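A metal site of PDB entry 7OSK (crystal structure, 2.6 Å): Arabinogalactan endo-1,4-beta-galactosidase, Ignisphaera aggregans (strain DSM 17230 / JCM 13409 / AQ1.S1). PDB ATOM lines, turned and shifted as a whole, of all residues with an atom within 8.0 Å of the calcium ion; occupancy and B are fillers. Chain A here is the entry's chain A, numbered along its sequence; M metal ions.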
ATOM      1  N   ASP A 300     -29.366  23.709   8.520  1.00  0.00           N
ATOM      2  CA  ASP A 300     -29.709  25.117   8.393  1.00  0.00           C
ATOM      3  C   ASP A 300     -29.304  25.705   7.047  1.00  0.00           C
ATOM      4  O   ASP A 300     -28.563  25.076   6.271  1.00  0.00           O
ATOM      5  CB  ASP A 300     -29.048  25.922   9.523  1.00  0.00           C
ATOM      6  CG  ASP A 300     -29.815  25.819  10.835  1.00  0.00           C
ATOM      7  OD1 ASP A 300     -30.558  24.833  11.020  1.00  0.00           O
ATOM      8  OD2 ASP A 300     -29.678  26.724  11.676  1.00  0.00           O
ATOM      9  N   ASP A 301     -29.805  26.901   6.753  1.00  0.00           N
ATOM     10  CA  ASP A 301     -29.493  27.619   5.524  1.00  0.00           C
ATOM     11  C   ASP A 301     -28.905  28.989   5.872  1.00  0.00           C
ATOM     12  O   ASP A 301     -29.210  29.547   6.927  1.00  0.00           O
ATOM     13  CB  ASP A 301     -30.737  27.781   4.647  1.00  0.00           C
ATOM     14  CG  ASP A 301     -30.424  28.354   3.278  1.00  0.00           C
ATOM     15  OD1 ASP A 301     -29.932  27.597   2.417  1.00  0.00           O
ATOM     16  OD2 ASP A 301     -30.682  29.553   3.061  1.00  0.00           O
ATOM     17  N   SER A 302     -28.087  29.531   4.975  1.00  0.00           N
ATOM     18  CA  SER A 302     -27.342  30.750   5.224  1.00  0.00           C
ATOM     19  C   SER A 302     -27.772  31.924   4.331  1.00  0.00           C
ATOM     20  O   SER A 302     -27.915  33.048   4.810  1.00  0.00           O
ATOM     21  CB  SER A 302     -25.846  30.494   5.031  1.00  0.00           C
ATOM     22  OG  SER A 302     -25.075  31.632   5.381  1.00  0.00           O
ATOM     23  N   ASP A 303     -27.955  31.650   3.044  1.00  0.00           N
ATOM     24  CA  ASP A 303     -28.152  32.707   2.051  1.00  0.00           C
ATOM     25  C   ASP A 303     -29.585  32.768   1.505  1.00  0.00           C
ATOM     26  O   ASP A 303     -29.851  33.483   0.536  1.00  0.00           O
ATOM     27  CB  ASP A 303     -27.169  32.510   0.893  1.00  0.00           C
ATOM     28  CG  ASP A 303     -27.228  31.122   0.279  1.00  0.00           C
ATOM     29  OD1 ASP A 303     -28.169  30.353   0.582  1.00  0.00           O
ATOM     30  OD2 ASP A 303     -26.330  30.797  -0.523  1.00  0.00           O
ATOM     31  N   GLY A 304     -30.497  32.027   2.119  1.00  0.00           N
ATOM     32  CA  GLY A 304     -31.890  32.048   1.715  1.00  0.00           C
ATOM     33  C   GLY A 304     -32.187  31.210   0.489  1.00  0.00           C
ATOM     34  O   GLY A 304     -33.350  31.103   0.080  1.00  0.00           O
ATOM     35  N   HIS A 305     -31.155  30.623  -0.095  1.00  0.00           N
ATOM     36  CA  HIS A 305     -31.325  29.736  -1.252  1.00  0.00           C
ATOM     37  C   HIS A 305     -31.399  28.288  -0.785  1.00  0.00           C
ATOM     38  O   HIS A 305     -30.403  27.737  -0.304  1.00  0.00           O
ATOM     39  CB  HIS A 305     -30.175  29.912  -2.242  1.00  0.00           C
ATOM     40  CG  HIS A 305     -30.307  29.072  -3.471  1.00  0.00           C
ATOM     41  ND1 HIS A 305     -30.890  29.530  -4.630  1.00  0.00           N
ATOM     42  CD2 HIS A 305     -29.943  27.789  -3.721  1.00  0.00           C
ATOM     43  CE1 HIS A 305     -30.871  28.578  -5.539  1.00  0.00           C
ATOM     44  NE2 HIS A 305     -30.310  27.510  -5.010  1.00  0.00           N
ATOM     45  N   PRO A 306     -32.581  27.650  -0.907  1.00  0.00           N
ATOM     46  CA  PRO A 306     -32.787  26.283  -0.420  1.00  0.00           C
ATOM     47  C   PRO A 306     -31.727  25.294  -0.880  1.00  0.00           C
ATOM     48  O   PRO A 306     -31.308  25.322  -2.038  1.00  0.00           O
ATOM     49  CB  PRO A 306     -34.154  25.897  -0.997  1.00  0.00           C
ATOM     50  CG  PRO A 306     -34.863  27.188  -1.148  1.00  0.00           C
ATOM     51  CD  PRO A 306     -33.816  28.188  -1.509  1.00  0.00           C
ATOM     52  N   ASN A 307     -31.291  24.425   0.027  1.00  0.00           N
ATOM     53  CA  ASN A 307     -30.242  23.458  -0.269  1.00  0.00           C
ATOM     54  C   ASN A 307     -30.803  22.114  -0.719  1.00  0.00           C
ATOM     55  O   ASN A 307     -31.966  21.798  -0.468  1.00  0.00           O
ATOM     56  CB  ASN A 307     -29.334  23.258   0.952  1.00  0.00           C
ATOM     57  CG  ASN A 307     -28.883  24.568   1.564  1.00  0.00           C
ATOM     58  OD1 ASN A 307     -28.200  25.370   0.916  1.00  0.00           O
ATOM     59  ND2 ASN A 307     -29.243  24.791   2.820  1.00  0.00           N
ATOM     60  N   ILE A 308     -29.958  21.334  -1.373  1.00  0.00           N
ATOM     61  CA  ILE A 308     -30.309  19.980  -1.800  1.00  0.00           C
ATOM     62  C   ILE A 308     -30.498  19.102  -0.565  1.00  0.00           C
ATOM     63  O   ILE A 308     -31.435  18.312  -0.487  1.00  0.00           O
ATOM     64  CB  ILE A 308     -29.224  19.412  -2.730  1.00  0.00           C
ATOM     65  CG1 ILE A 308     -29.404  19.991  -4.132  1.00  0.00           C
ATOM     66  CG2 ILE A 308     -29.282  17.886  -2.784  1.00  0.00           C
ATOM     67  CD1 ILE A 308     -28.134  20.057  -4.950  1.00  0.00           C
ATOM     68  N   PRO A 358     -20.941  30.031   1.625  1.00  0.00           N
ATOM     69  CA  PRO A 358     -21.908  30.997   1.119  1.00  0.00           C
ATOM     70  C   PRO A 358     -21.282  32.372   0.924  1.00  0.00           C
ATOM     71  O   PRO A 358     -20.699  32.915   1.867  1.00  0.00           O
ATOM     72  CB  PRO A 358     -22.972  31.025   2.215  1.00  0.00           C
ATOM     73  CG  PRO A 358     -22.234  30.674   3.459  1.00  0.00           C
ATOM     74  CD  PRO A 358     -21.162  29.712   3.050  1.00  0.00           C
ATOM     75  N   GLY A 369     -28.287  31.435  -5.704  1.00  0.00           N
ATOM     76  CA  GLY A 369     -27.431  31.251  -4.549  1.00  0.00           C
ATOM     77  C   GLY A 369     -26.818  29.873  -4.405  1.00  0.00           C
ATOM     78  O   GLY A 369     -26.711  29.122  -5.368  1.00  0.00           O
ATOM     79  N   ASN A 370     -26.419  29.559  -3.170  1.00  0.00           N
ATOM     80  CA  ASN A 370     -25.752  28.301  -2.863  1.00  0.00           C
ATOM     81  C   ASN A 370     -26.715  27.248  -2.313  1.00  0.00           C
ATOM     82  O   ASN A 370     -27.425  27.506  -1.348  1.00  0.00           O
ATOM     83  CB  ASN A 370     -24.630  28.547  -1.855  1.00  0.00           C
ATOM     84  CG  ASN A 370     -23.616  27.414  -1.815  1.00  0.00           C
ATOM     85  OD1 ASN A 370     -23.915  26.289  -2.207  1.00  0.00           O
ATOM     86  ND2 ASN A 370     -22.413  27.717  -1.349  1.00  0.00           N
ATOM     87  N   PRO A 371     -26.745  26.044  -2.931  1.00  0.00           N
ATOM     88  CA  PRO A 371     -27.567  24.950  -2.411  1.00  0.00           C
ATOM     89  C   PRO A 371     -26.758  23.878  -1.681  1.00  0.00           C
ATOM     90  O   PRO A 371     -27.281  22.782  -1.464  1.00  0.00           O
ATOM     91  CB  PRO A 371     -28.181  24.372  -3.686  1.00  0.00           C
ATOM     92  CG  PRO A 371     -27.059  24.506  -4.691  1.00  0.00           C
ATOM     93  CD  PRO A 371     -26.277  25.752  -4.304  1.00  0.00           C
ATOM     94  N   TRP A 372     -25.518  24.189  -1.311  1.00  0.00           N
ATOM     95  CA  TRP A 372     -24.575  23.170  -0.865  1.00  0.00           C
ATOM     96  C   TRP A 372     -23.788  23.549   0.396  1.00  0.00           C
ATOM     97  O   TRP A 372     -23.002  22.747   0.905  1.00  0.00           O
ATOM     98  CB  TRP A 372     -23.608  22.860  -2.007  1.00  0.00           C
ATOM     99  CG  TRP A 372     -22.921  21.524  -1.894  1.00  0.00           C
ATOM    100  CD1 TRP A 372     -21.686  21.281  -1.393  1.00  0.00           C
ATOM    101  CD2 TRP A 372     -23.443  20.257  -2.308  1.00  0.00           C
ATOM    102  NE1 TRP A 372     -21.401  19.940  -1.463  1.00  0.00           N
ATOM    103  CE2 TRP A 372     -22.472  19.292  -2.026  1.00  0.00           C
ATOM    104  CE3 TRP A 372     -24.646  19.846  -2.890  1.00  0.00           C
ATOM    105  CZ2 TRP A 372     -22.648  17.936  -2.301  1.00  0.00           C
ATOM    106  CZ3 TRP A 372     -24.831  18.508  -3.161  1.00  0.00           C
ATOM    107  CH2 TRP A 372     -23.835  17.564  -2.874  1.00  0.00           C
ATOM    108  N   GLU A 373     -23.994  24.761   0.904  1.00  0.00           N
ATOM    109  CA  GLU A 373     -23.118  25.291   1.948  1.00  0.00           C
ATOM    110  C   GLU A 373     -23.192  24.473   3.245  1.00  0.00           C
ATOM    111  O   GLU A 373     -22.248  24.498   4.040  1.00  0.00           O
ATOM    112  CB  GLU A 373     -23.457  26.767   2.239  1.00  0.00           C
ATOM    113  CG  GLU A 373     -24.726  27.043   3.045  1.00  0.00           C
ATOM    114  CD  GLU A 373     -25.939  27.383   2.195  1.00  0.00           C
ATOM    115  OE1 GLU A 373     -25.890  27.226   0.956  1.00  0.00           O
ATOM    116  OE2 GLU A 373     -26.947  27.821   2.790  1.00  0.00           O
ATOM    117  N   ASN A 374     -24.287  23.761   3.447  1.00  0.00           N
ATOM    118  CA  ASN A 374     -24.429  22.918   4.628  1.00  0.00           C
ATOM    119  C   ASN A 374     -23.766  21.560   4.418  1.00  0.00           C
ATOM    120  O   ASN A 374     -23.863  20.673   5.272  1.00  0.00           O
ATOM    121  CB  ASN A 374     -25.901  22.731   5.016  1.00  0.00           C
ATOM    122  CG  ASN A 374     -26.692  21.971   3.966  1.00  0.00           C
ATOM    123  OD1 ASN A 374     -26.467  22.123   2.769  1.00  0.00           O
ATOM    124  ND2 ASN A 374     -27.645  21.158   4.428  1.00  0.00           N
ATOM    125  N   PHE A 380     -20.504  28.870   7.456  1.00  0.00           N
ATOM    126  CA  PHE A 380     -20.981  30.017   6.673  1.00  0.00           C
ATOM    127  C   PHE A 380     -20.032  31.203   6.797  1.00  0.00           C
ATOM    128  O   PHE A 380     -19.940  32.023   5.885  1.00  0.00           O
ATOM    129  CB  PHE A 380     -22.388  30.406   7.134  1.00  0.00           C
ATOM    130  CG  PHE A 380     -23.368  29.264   7.141  1.00  0.00           C
ATOM    131  CD1 PHE A 380     -23.186  28.178   6.303  1.00  0.00           C
ATOM    132  CD2 PHE A 380     -24.460  29.273   7.990  1.00  0.00           C
ATOM    133  CE1 PHE A 380     -24.074  27.124   6.308  1.00  0.00           C
ATOM    134  CE2 PHE A 380     -25.359  28.216   7.989  1.00  0.00           C
ATOM    135  CZ  PHE A 380     -25.161  27.147   7.157  1.00  0.00           C
HETATM  136 CA    CA M   1     -28.179  27.865   0.817  1.00  0.00          CA
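Of the 17 residues printed, 6 come within 4 Å of the calcium ion.
The side-chain carboxylate (OD2) of Asp 301 sits at hydrogen-bond distance from the backbone NH (N) of Gly 304, at 2.7 Å.
OE2 of Glu 373 lies close to N of Ser 302, at 3.0 Å.
The backbone NH (N) of Trp 372 is in hydrogen-bond range of the side-chain amide oxygen (OD1) of Asn 370, 2.8 Å away.
ND1 of His 305 lies within hydrogen-bond range of N of Gly 369, 3.4 Å away.
The calcium ion is bound by the backbone carbonyl oxygen (O) of Asn 370, the side-chain carboxylate (OE2) of Glu 373, the side-chain carboxylate (OE1) of Glu 373, the side-chain carboxylate (OD1) of Asp 301, the backbone carbonyl oxygen (O) of His 305, the side-chain amide oxygen (OD1) of Asn 307 and the side-chain carboxylate (OD1) of Asp 303.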
